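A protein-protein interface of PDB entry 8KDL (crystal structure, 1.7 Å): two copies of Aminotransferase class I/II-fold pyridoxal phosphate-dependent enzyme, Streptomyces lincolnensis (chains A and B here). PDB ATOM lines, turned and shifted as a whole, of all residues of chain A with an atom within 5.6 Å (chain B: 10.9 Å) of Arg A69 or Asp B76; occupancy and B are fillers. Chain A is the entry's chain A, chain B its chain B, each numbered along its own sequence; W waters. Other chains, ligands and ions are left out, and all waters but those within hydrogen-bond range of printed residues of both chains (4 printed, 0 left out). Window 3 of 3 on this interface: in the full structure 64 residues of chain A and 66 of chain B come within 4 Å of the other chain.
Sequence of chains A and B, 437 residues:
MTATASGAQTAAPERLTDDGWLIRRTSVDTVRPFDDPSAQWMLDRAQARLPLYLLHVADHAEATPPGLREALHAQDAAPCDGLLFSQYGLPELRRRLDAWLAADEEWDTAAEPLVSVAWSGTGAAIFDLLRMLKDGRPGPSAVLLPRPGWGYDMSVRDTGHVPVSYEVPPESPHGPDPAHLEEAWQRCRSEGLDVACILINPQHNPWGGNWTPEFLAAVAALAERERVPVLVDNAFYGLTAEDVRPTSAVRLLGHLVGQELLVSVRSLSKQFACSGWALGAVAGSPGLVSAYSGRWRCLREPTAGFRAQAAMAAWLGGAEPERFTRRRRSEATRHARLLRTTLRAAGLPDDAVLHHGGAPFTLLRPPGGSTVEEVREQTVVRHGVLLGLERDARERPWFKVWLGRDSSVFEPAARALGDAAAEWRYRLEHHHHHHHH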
ATOM      1  N   THR A  64      15.476   3.799 -14.135  1.00  0.00           N
ATOM      2  CA  THR A  64      16.533   4.592 -13.524  1.00  0.00           C
ATOM      3  C   THR A  64      17.889   3.931 -13.747  1.00  0.00           C
ATOM      4  O   THR A  64      17.974   2.778 -14.169  1.00  0.00           O
ATOM      5  CB  THR A  64      16.256   4.726 -12.032  1.00  0.00           C
ATOM      6  OG1 THR A  64      16.088   3.413 -11.482  1.00  0.00           O
ATOM      7  CG2 THR A  64      15.005   5.545 -11.802  1.00  0.00           C
ATOM      8  N   PRO A  65      18.993   4.637 -13.480  1.00  0.00           N
ATOM      9  CA  PRO A  65      20.323   4.030 -13.660  1.00  0.00           C
ATOM     10  C   PRO A  65      20.591   3.005 -12.575  1.00  0.00           C
ATOM     11  O   PRO A  65      20.039   3.120 -11.468  1.00  0.00           O
ATOM     12  CB  PRO A  65      21.279   5.222 -13.508  1.00  0.00           C
ATOM     13  CG  PRO A  65      20.463   6.395 -13.793  1.00  0.00           C
ATOM     14  CD  PRO A  65      19.099   6.091 -13.267  1.00  0.00           C
ATOM     15  N   GLY A  67      21.784   1.331  -9.376  1.00  0.00           N
ATOM     16  CA  GLY A  67      22.221   1.822  -8.080  1.00  0.00           C
ATOM     17  C   GLY A  67      21.433   2.994  -7.533  1.00  0.00           C
ATOM     18  O   GLY A  67      21.523   3.276  -6.335  1.00  0.00           O
ATOM     19  N   LEU A  68      20.669   3.693  -8.373  1.00  0.00           N
ATOM     20  CA  LEU A  68      20.036   4.925  -7.916  1.00  0.00           C
ATOM     21  C   LEU A  68      18.860   4.639  -6.985  1.00  0.00           C
ATOM     22  O   LEU A  68      18.727   5.276  -5.936  1.00  0.00           O
ATOM     23  CB  LEU A  68      19.605   5.764  -9.119  1.00  0.00           C
ATOM     24  CG  LEU A  68      19.014   7.117  -8.701  1.00  0.00           C
ATOM     25  CD1 LEU A  68      20.073   7.945  -8.004  1.00  0.00           C
ATOM     26  CD2 LEU A  68      18.447   7.891  -9.878  1.00  0.00           C
ATOM     27  N   ARG A  69      17.994   3.681  -7.339  1.00  0.00           N
ATOM     28  CA  ARG A  69      16.903   3.327  -6.430  1.00  0.00           C
ATOM     29  C   ARG A  69      17.435   2.725  -5.136  1.00  0.00           C
ATOM     30  O   ARG A  69      16.899   2.992  -4.055  1.00  0.00           O
ATOM     31  CB  ARG A  69      15.944   2.355  -7.106  1.00  0.00           C
ATOM     32  CG  ARG A  69      15.232   2.937  -8.292  1.00  0.00           C
ATOM     33  CD  ARG A  69      14.283   1.867  -8.824  1.00  0.00           C
ATOM     34  NE  ARG A  69      15.007   0.673  -9.237  1.00  0.00           N
ATOM     35  CZ  ARG A  69      14.432  -0.440  -9.672  1.00  0.00           C
ATOM     36  NH1 ARG A  69      13.116  -0.584  -9.672  1.00  0.00           N
ATOM     37  NH2 ARG A  69      15.197  -1.433 -10.117  1.00  0.00           N
ATOM     38  N   GLU A  70      18.505   1.931  -5.223  1.00  0.00           N
ATOM     39  CA  GLU A  70      19.123   1.405  -4.013  1.00  0.00           C
ATOM     40  C   GLU A  70      19.596   2.536  -3.101  1.00  0.00           C
ATOM     41  O   GLU A  70      19.527   2.414  -1.872  1.00  0.00           O
ATOM     42  CB  GLU A  70      20.287   0.482  -4.384  1.00  0.00           C
ATOM     43  CG  GLU A  70      19.913  -0.827  -5.095  1.00  0.00           C
ATOM     44  CD  GLU A  70      19.675  -0.707  -6.611  1.00  0.00           C
ATOM     45  OE1 GLU A  70      19.621   0.414  -7.173  1.00  0.00           O
ATOM     46  OE2 GLU A  70      19.586  -1.776  -7.264  1.00  0.00           O
ATOM     47  N   ALA A  71      20.063   3.648  -3.686  1.00  0.00           N
ATOM     48  CA  ALA A  71      20.518   4.774  -2.877  1.00  0.00           C
ATOM     49  C   ALA A  71      19.375   5.366  -2.061  1.00  0.00           C
ATOM     50  O   ALA A  71      19.579   5.789  -0.913  1.00  0.00           O
ATOM     51  CB  ALA A  71      21.159   5.842  -3.770  1.00  0.00           C
ATOM     52  N   LEU A  72      18.156   5.385  -2.613  1.00  0.00           N
ATOM     53  CA  LEU A  72      17.024   5.841  -1.801  1.00  0.00           C
ATOM     54  C   LEU A  72      16.801   4.959  -0.584  1.00  0.00           C
ATOM     55  O   LEU A  72      16.427   5.459   0.485  1.00  0.00           O
ATOM     56  CB  LEU A  72      15.722   5.898  -2.600  1.00  0.00           C
ATOM     57  CG  LEU A  72      15.399   6.980  -3.600  1.00  0.00           C
ATOM     58  CD1 LEU A  72      14.039   6.604  -4.187  1.00  0.00           C
ATOM     59  CD2 LEU A  72      15.340   8.350  -2.921  1.00  0.00           C
ATOM     60  N   HIS A  73      16.966   3.637  -0.736  1.00  0.00           N
ATOM     61  CA  HIS A  73      16.823   2.732   0.406  1.00  0.00           C
ATOM     62  C   HIS A  73      17.896   2.982   1.453  1.00  0.00           C
ATOM     63  O   HIS A  73      17.623   2.926   2.659  1.00  0.00           O
ATOM     64  CB  HIS A  73      16.926   1.260  -0.007  1.00  0.00           C
ATOM     65  CG  HIS A  73      15.777   0.742  -0.810  1.00  0.00           C
ATOM     66  ND1 HIS A  73      15.177  -0.472  -0.532  1.00  0.00           N
ATOM     67  CD2 HIS A  73      15.166   1.220  -1.918  1.00  0.00           C
ATOM     68  CE1 HIS A  73      14.215  -0.695  -1.411  1.00  0.00           C
ATOM     69  NE2 HIS A  73      14.190   0.315  -2.265  1.00  0.00           N
ATOM     70  N   ALA A  74      19.143   3.167   1.013  1.00  0.00           N
ATOM     71  CA  ALA A  74      20.245   3.312   1.952  1.00  0.00           C
ATOM     72  C   ALA A  74      20.022   4.493   2.879  1.00  0.00           C
ATOM     73  O   ALA A  74      20.482   4.473   4.021  1.00  0.00           O
ATOM     74  CB  ALA A  74      21.571   3.467   1.204  1.00  0.00           C
ATOM     75  N   TRP A 277      12.513  13.176  -9.712  1.00  0.00           N
ATOM     76  CA  TRP A 277      13.207  13.735  -8.561  1.00  0.00           C
ATOM     77  C   TRP A 277      13.476  15.230  -8.710  1.00  0.00           C
ATOM     78  O   TRP A 277      13.784  15.891  -7.713  1.00  0.00           O
ATOM     79  CB  TRP A 277      14.530  13.002  -8.343  1.00  0.00           C
ATOM     80  CG  TRP A 277      14.462  11.517  -8.042  1.00  0.00           C
ATOM     81  CD1 TRP A 277      13.463  10.631  -8.356  1.00  0.00           C
ATOM     82  CD2 TRP A 277      15.483  10.755  -7.400  1.00  0.00           C
ATOM     83  NE1 TRP A 277      13.799   9.366  -7.927  1.00  0.00           N
ATOM     84  CE2 TRP A 277      15.042   9.414  -7.347  1.00  0.00           C
ATOM     85  CE3 TRP A 277      16.733  11.085  -6.837  1.00  0.00           C
ATOM     86  CZ2 TRP A 277      15.805   8.397  -6.761  1.00  0.00           C
ATOM     87  CZ3 TRP A 277      17.501  10.066  -6.272  1.00  0.00           C
ATOM     88  CH2 TRP A 277      17.030   8.739  -6.238  1.00  0.00           C
ATOM     89  N   LEU B  68       5.613   4.503   5.969  1.00  0.00           N
ATOM     90  CA  LEU B  68       5.738   5.427   4.841  1.00  0.00           C
ATOM     91  C   LEU B  68       7.014   5.177   4.037  1.00  0.00           C
ATOM     92  O   LEU B  68       6.974   5.161   2.803  1.00  0.00           O
ATOM     93  CB  LEU B  68       5.689   6.882   5.335  1.00  0.00           C
ATOM     94  CG  LEU B  68       5.732   7.919   4.196  1.00  0.00           C
ATOM     95  CD1 LEU B  68       4.503   7.739   3.327  1.00  0.00           C
ATOM     96  CD2 LEU B  68       5.803   9.363   4.701  1.00  0.00           C
ATOM     97  N   ARG B  69       8.162   4.984   4.708  1.00  0.00           N
ATOM     98  CA  ARG B  69       9.388   4.692   3.964  1.00  0.00           C
ATOM     99  C   ARG B  69       9.301   3.331   3.287  1.00  0.00           C
ATOM    100  O   ARG B  69       9.840   3.137   2.191  1.00  0.00           O
ATOM    101  CB  ARG B  69      10.602   4.731   4.888  1.00  0.00           C
ATOM    102  CG  ARG B  69      10.872   6.091   5.512  1.00  0.00           C
ATOM    103  CD  ARG B  69      12.069   5.946   6.444  1.00  0.00           C
ATOM    104  NE  ARG B  69      11.761   5.008   7.521  1.00  0.00           N
ATOM    105  CZ  ARG B  69      12.651   4.549   8.385  1.00  0.00           C
ATOM    106  NH1 ARG B  69      13.928   4.882   8.299  1.00  0.00           N
ATOM    107  NH2 ARG B  69      12.256   3.703   9.335  1.00  0.00           N
ATOM    108  N   GLU B  70       8.642   2.372   3.945  1.00  0.00           N
ATOM    109  CA  GLU B  70       8.407   1.081   3.324  1.00  0.00           C
ATOM    110  C   GLU B  70       7.599   1.238   2.046  1.00  0.00           C
ATOM    111  O   GLU B  70       7.898   0.593   1.027  1.00  0.00           O
ATOM    112  CB  GLU B  70       7.686   0.153   4.302  1.00  0.00           C
ATOM    113  CG  GLU B  70       8.507  -0.314   5.502  1.00  0.00           C
ATOM    114  CD  GLU B  70       8.533   0.667   6.665  1.00  0.00           C
ATOM    115  OE1 GLU B  70       8.037   1.818   6.544  1.00  0.00           O
ATOM    116  OE2 GLU B  70       9.031   0.259   7.739  1.00  0.00           O
ATOM    117  N   ALA B  71       6.559   2.084   2.086  1.00  0.00           N
ATOM    118  CA  ALA B  71       5.760   2.334   0.889  1.00  0.00           C
ATOM    119  C   ALA B  71       6.618   2.923  -0.223  1.00  0.00           C
ATOM    120  O   ALA B  71       6.434   2.599  -1.405  1.00  0.00           O
ATOM    121  CB  ALA B  71       4.586   3.264   1.219  1.00  0.00           C
ATOM    122  N   LEU B  72       7.584   3.773   0.137  1.00  0.00           N
ATOM    123  CA  LEU B  72       8.466   4.354  -0.871  1.00  0.00           C
ATOM    124  C   LEU B  72       9.304   3.280  -1.557  1.00  0.00           C
ATOM    125  O   LEU B  72       9.469   3.291  -2.787  1.00  0.00           O
ATOM    126  CB  LEU B  72       9.362   5.401  -0.213  1.00  0.00           C
ATOM    127  CG  LEU B  72      10.103   6.333  -1.180  1.00  0.00           C
ATOM    128  CD1 LEU B  72       9.159   7.285  -1.894  1.00  0.00           C
ATOM    129  CD2 LEU B  72      11.205   7.078  -0.449  1.00  0.00           C
ATOM    130  N   HIS B  73       9.830   2.343  -0.772  1.00  0.00           N
ATOM    131  CA  HIS B  73      10.651   1.268  -1.317  1.00  0.00           C
ATOM    132  C   HIS B  73       9.821   0.293  -2.137  1.00  0.00           C
ATOM    133  O   HIS B  73      10.312  -0.263  -3.131  1.00  0.00           O
ATOM    134  CB  HIS B  73      11.362   0.526  -0.185  1.00  0.00           C
ATOM    135  CG  HIS B  73      12.088   1.421   0.766  1.00  0.00           C
ATOM    136  ND1 HIS B  73      12.675   2.607   0.373  1.00  0.00           N
ATOM    137  CD2 HIS B  73      12.327   1.305   2.095  1.00  0.00           C
ATOM    138  CE1 HIS B  73      13.238   3.185   1.420  1.00  0.00           C
ATOM    139  NE2 HIS B  73      13.052   2.409   2.474  1.00  0.00           N
ATOM    140  N   ALA B  74       8.570   0.050  -1.717  1.00  0.00           N
ATOM    141  CA  ALA B  74       7.707  -0.897  -2.419  1.00  0.00           C
ATOM    142  C   ALA B  74       7.414  -0.442  -3.841  1.00  0.00           C
ATOM    143  O   ALA B  74       7.149  -1.274  -4.720  1.00  0.00           O
ATOM    144  CB  ALA B  74       6.396  -1.096  -1.646  1.00  0.00           C
ATOM    145  N   GLN B  75       7.464   0.862  -4.089  1.00  0.00           N
ATOM    146  CA  GLN B  75       7.250   1.340  -5.448  1.00  0.00           C
ATOM    147  C   GLN B  75       8.392   0.967  -6.399  1.00  0.00           C
ATOM    148  O   GLN B  75       8.255   1.224  -7.596  1.00  0.00           O
ATOM    149  CB  GLN B  75       7.006   2.862  -5.440  1.00  0.00           C
ATOM    150  CG  GLN B  75       5.695   3.241  -4.734  1.00  0.00           C
ATOM    151  CD  GLN B  75       4.476   2.638  -5.447  1.00  0.00           C
ATOM    152  OE1 GLN B  75       4.412   2.653  -6.676  1.00  0.00           O
ATOM    153  NE2 GLN B  75       3.543   2.065  -4.678  1.00  0.00           N
ATOM    154  N   ASP B  76       9.481   0.325  -5.936  1.00  0.00           N
ATOM    155  CA  ASP B  76      10.430  -0.273  -6.885  1.00  0.00           C
ATOM    156  C   ASP B  76       9.774  -1.292  -7.816  1.00  0.00           C
ATOM    157  O   ASP B  76      10.387  -1.666  -8.826  1.00  0.00           O
ATOM    158  CB  ASP B  76      11.582  -0.988  -6.161  1.00  0.00           C
ATOM    159  CG  ASP B  76      12.523  -0.038  -5.446  1.00  0.00           C
ATOM    160  OD1 ASP B  76      12.402   1.183  -5.651  1.00  0.00           O
ATOM    161  OD2 ASP B  76      13.429  -0.536  -4.713  1.00  0.00           O
ATOM    162  N   ALA B  77       8.553  -1.740  -7.503  1.00  0.00           N
ATOM    163  CA  ALA B  77       7.904  -2.811  -8.257  1.00  0.00           C
ATOM    164  C   ALA B  77       7.653  -2.440  -9.712  1.00  0.00           C
ATOM    165  O   ALA B  77       7.509  -3.333 -10.563  1.00  0.00           O
ATOM    166  CB  ALA B  77       6.580  -3.181  -7.581  1.00  0.00           C
ATOM    167  N   ALA B  78       7.585  -1.152 -10.016  1.00  0.00           N
ATOM    168  CA  ALA B  78       7.326  -0.684 -11.370  1.00  0.00           C
ATOM    169  C   ALA B  78       8.089   0.618 -11.566  1.00  0.00           C
ATOM    170  O   ALA B  78       8.397   1.309 -10.590  1.00  0.00           O
ATOM    171  CB  ALA B  78       5.822  -0.478 -11.599  1.00  0.00           C
ATOM    172  N   PRO B  79       8.418   0.976 -12.810  1.00  0.00           N
ATOM    173  CA  PRO B  79       9.181   2.219 -13.049  1.00  0.00           C
ATOM    174  C   PRO B  79       8.321   3.415 -12.676  1.00  0.00           C
ATOM    175  O   PRO B  79       7.218   3.595 -13.204  1.00  0.00           O
ATOM    176  CB  PRO B  79       9.492   2.184 -14.551  1.00  0.00           C
ATOM    177  CG  PRO B  79       8.746   1.018 -15.125  1.00  0.00           C
ATOM    178  CD  PRO B  79       8.146   0.207 -14.040  1.00  0.00           C
ATOM    179  N   CYS B  80       8.826   4.232 -11.757  1.00  0.00           N
ATOM    180  CA  CYS B  80       8.008   5.307 -11.212  1.00  0.00           C
ATOM    181  C   CYS B  80       8.841   6.553 -10.936  1.00  0.00           C
ATOM    182  O   CYS B  80       8.537   7.306 -10.010  1.00  0.00           O
ATOM    183  CB  CYS B  80       7.311   4.881  -9.913  1.00  0.00           C
ATOM    184  SG  CYS B  80       8.478   4.438  -8.594  1.00  0.00           S
ATOM    185  N   ASP B  81       9.908   6.773 -11.703  1.00  0.00           N
ATOM    186  CA  ASP B  81      10.724   7.963 -11.516  1.00  0.00           C
ATOM    187  C   ASP B  81      10.786   8.836 -12.759  1.00  0.00           C
ATOM    188  O   ASP B  81      11.633   9.740 -12.822  1.00  0.00           O
ATOM    189  CB  ASP B  81      12.128   7.565 -11.060  1.00  0.00           C
ATOM    190  CG  ASP B  81      12.108   6.883  -9.707  1.00  0.00           C
ATOM    191  OD1 ASP B  81      11.796   7.562  -8.702  1.00  0.00           O
ATOM    192  OD2 ASP B  81      12.351   5.655  -9.662  1.00  0.00           O
ATOM    193  N   GLY B  82       9.902   8.593 -13.738  1.00  0.00           N
ATOM    194  CA  GLY B  82       9.763   9.459 -14.891  1.00  0.00           C
ATOM    195  C   GLY B  82       8.744  10.565 -14.630  1.00  0.00           C
ATOM    196  O   GLY B  82       8.125  10.645 -13.573  1.00  0.00           O
ATOM    197  N   GLU B  92      -3.750   7.794  -8.950  1.00  0.00           N
ATOM    198  CA  GLU B  92      -4.048   6.997  -7.759  1.00  0.00           C
ATOM    199  C   GLU B  92      -3.934   7.832  -6.485  1.00  0.00           C
ATOM    200  O   GLU B  92      -4.642   7.564  -5.507  1.00  0.00           O
ATOM    201  CB  GLU B  92      -3.131   5.763  -7.674  1.00  0.00           C
ATOM    202  CG  GLU B  92      -1.661   6.084  -7.807  1.00  0.00           C
ATOM    203  CD  GLU B  92      -0.830   4.895  -8.253  1.00  0.00           C
ATOM    204  OE1 GLU B  92      -0.829   4.637  -9.464  1.00  0.00           O
ATOM    205  OE2 GLU B  92      -0.099   4.294  -7.441  1.00  0.00           O
ATOM    206  N   PHE B 306       6.560  11.425  -9.166  1.00  0.00           N
ATOM    207  CA  PHE B 306       5.875  10.161  -9.438  1.00  0.00           C
ATOM    208  C   PHE B 306       5.989   9.178  -8.260  1.00  0.00           C
ATOM    209  O   PHE B 306       4.972   8.740  -7.701  1.00  0.00           O
ATOM    210  CB  PHE B 306       6.441   9.602 -10.753  1.00  0.00           C
ATOM    211  CG  PHE B 306       5.721   8.397 -11.316  1.00  0.00           C
ATOM    212  CD1 PHE B 306       4.760   7.688 -10.605  1.00  0.00           C
ATOM    213  CD2 PHE B 306       6.002   8.007 -12.626  1.00  0.00           C
ATOM    214  CE1 PHE B 306       4.126   6.563 -11.183  1.00  0.00           C
ATOM    215  CE2 PHE B 306       5.383   6.914 -13.209  1.00  0.00           C
ATOM    216  CZ  PHE B 306       4.439   6.182 -12.485  1.00  0.00           C
ATOM    217  N   ARG B 307       7.219   8.859  -7.832  1.00  0.00           N
ATOM    218  CA  ARG B 307       7.402   7.840  -6.795  1.00  0.00           C
ATOM    219  C   ARG B 307       6.791   8.278  -5.472  1.00  0.00           C
ATOM    220  O   ARG B 307       6.115   7.494  -4.793  1.00  0.00           O
ATOM    221  CB  ARG B 307       8.886   7.540  -6.593  1.00  0.00           C
ATOM    222  CG  ARG B 307       9.149   6.532  -5.460  1.00  0.00           C
ATOM    223  CD  ARG B 307      10.652   6.338  -5.263  1.00  0.00           C
ATOM    224  NE  ARG B 307      11.228   5.665  -6.415  1.00  0.00           N
ATOM    225  CZ  ARG B 307      11.309   4.347  -6.526  1.00  0.00           C
ATOM    226  NH1 ARG B 307      10.839   3.545  -5.577  1.00  0.00           N
ATOM    227  NH2 ARG B 307      11.886   3.819  -7.604  1.00  0.00           N
ATOM    228  N   ALA B 308       7.041   9.524  -5.077  1.00  0.00           N
ATOM    229  CA  ALA B 308       6.510   9.993  -3.799  1.00  0.00           C
ATOM    230  C   ALA B 308       4.986   9.973  -3.804  1.00  0.00           C
ATOM    231  O   ALA B 308       4.341   9.575  -2.818  1.00  0.00           O
ATOM    232  CB  ALA B 308       7.055  11.394  -3.510  1.00  0.00           C
ATOM    233  N   ALA B 310       3.044   7.989  -5.591  1.00  0.00           N
ATOM    234  CA  ALA B 310       2.572   6.604  -5.590  1.00  0.00           C
ATOM    235  C   ALA B 310       2.694   5.992  -4.207  1.00  0.00           C
ATOM    236  O   ALA B 310       1.781   5.298  -3.732  1.00  0.00           O
ATOM    237  CB  ALA B 310       3.379   5.779  -6.595  1.00  0.00           C
ATOM    238  N   ALA B 311       3.824   6.247  -3.556  1.00  0.00           N
ATOM    239  CA  ALA B 311       4.027   5.791  -2.191  1.00  0.00           C
ATOM    240  C   ALA B 311       2.984   6.402  -1.265  1.00  0.00           C
ATOM    241  O   ALA B 311       2.384   5.706  -0.440  1.00  0.00           O
ATOM    242  CB  ALA B 311       5.447   6.152  -1.753  1.00  0.00           C
ATOM    243  N   ALA B 314      -0.516   4.788  -1.723  1.00  0.00           N
ATOM    244  CA  ALA B 314      -0.592   3.506  -1.032  1.00  0.00           C
ATOM    245  C   ALA B 314      -0.639   3.694   0.478  1.00  0.00           C
ATOM    246  O   ALA B 314      -1.456   3.058   1.162  1.00  0.00           O
ATOM    247  CB  ALA B 314       0.605   2.641  -1.413  1.00  0.00           C
HETATM  248  O   HOH W   1      13.916   2.860  -4.091  1.00  0.00           O
HETATM  249  O   HOH W   2      10.453  -1.696 -11.595  1.00  0.00           O
HETATM  250  O   HOH W   3      16.153  -0.571  -4.964  1.00  0.00           O
HETATM  251  O   HOH W   4      11.085   1.696  -9.676  1.00  0.00           O
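NE2 of His A73 is in hydrogen-bond range of OD2 of Asp B76 (2.7 Å).
NE1 of Trp A277 lies within hydrogen-bond range of OD1 of Asp B81 (2.8 Å).
NH1 of Arg A69 sits at hydrogen-bond distance from O of Asp B76 (3.1 Å).
The side-chain carboxylate of Asp B76 is in salt-bridge range of the guanidinium group of Arg B307, 2.8 Å away.
OD2 of Asp B81 lies within salt-bridge range of NH2 of Arg B307.
O of Arg B69 lies close to NE2 of His B73, 3.3 Å away.
The backbone carbonyl oxygen (O) of Leu B72 is in hydrogen-bond range of the guanidinium group (NH1) of Arg B307, 3.1 Å away.
N of Arg B307 is in hydrogen-bond range of O of Cys B80, at 3.0 Å.
Among the printed residues, pairs that only touch across the chains: Thr A64 with Asp B81 (3.4 Å), Arg A69 with Arg B307 (3.3 Å), Leu A72 with Arg B307 (3.6 Å) and His A73 with His B73 (3.3 Å).
Of chain B, only Asp B76 (3.1 Å) and Arg B307 (3.3 Å) come within 4 Å of Arg A69.
Asp B76 touches just these residues of chain A: Arg A69 and His A73.
Of chain B, only Asp B81 (3.4 Å) comes within 4 Å of Thr A64.
No residue of chain B comes within 4 Å of Gly A67.
No residue of chain B comes within 4 Å of Leu A68.
No residue of chain B comes within 4 Å of Glu A70.
No residue of chain B comes within 4 Å of Ala A71.
Leu A72 touches just one residue of chain B: Arg B307 (3.6 Å).
Of the printed residues of chain A, Arg B307 touches Arg A69 and Leu A72.
Printed residues of chain B within 4 Å of Trp A277: Asp B81.
Of the printed residues of chain A, His B73 touches His A73 (3.3 Å).
Ala B308 touches none of the printed residues of chain A.
Glu B92 touches none of the printed residues of chain A.
The nearest residue of chain B that does not touch Arg A69 is Asp B81 (4.2 Å).
The nearest printed residue of chain A that does not touch Asp B76 is Glu A70 (5.7 Å).
Of the 11 printed residues of chain A, 5 touch a printed residue of chain B.
Of the 22 printed residues of chain B, 4 touch a printed residue of chain A.
Hydrophobic or aromatic side chains of chain B that line the printed part of chain A: His B73.
Among the printed residues, no Asp or Glu carboxylate lies within 4 Å of a Lys or Arg side-chain nitrogen of the other chain.
His B73 touches its own counterpart, His A73.
Positions printed for both chains: 68, 69, 70, 71, 72, 73 and 74.
Water W3 lies within hydrogen-bond range of the side-chain carboxylate of Asp B76 (2.7 Å), the backbone NH of Glu A70 (3.4 Å) and a ring nitrogen (NE2) of His A73 (3.5 Å).
Water W1 lies within hydrogen-bond range of the side-chain carboxylate of Asp B76 (2.7 Å), the backbone carbonyl oxygen of Arg A69 (3.0 Å), a ring nitrogen (NE2) of His A73 (3.1 Å) and the guanidinium group of Arg B307 (3.5 Å).
Water W2 lies within hydrogen-bond range of the backbone carbonyl oxygen of Asp B76 (2.8 Å), the backbone NH of Ala B78 (3.3 Å) and the guanidinium group of Arg A69 (3.5 Å).
Water W4 lies within hydrogen-bond range of O of Ala B78 (2.9 Å), NH1 of Arg A69 (3.1 Å) and NH2 of Arg B307 (3.1 Å).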
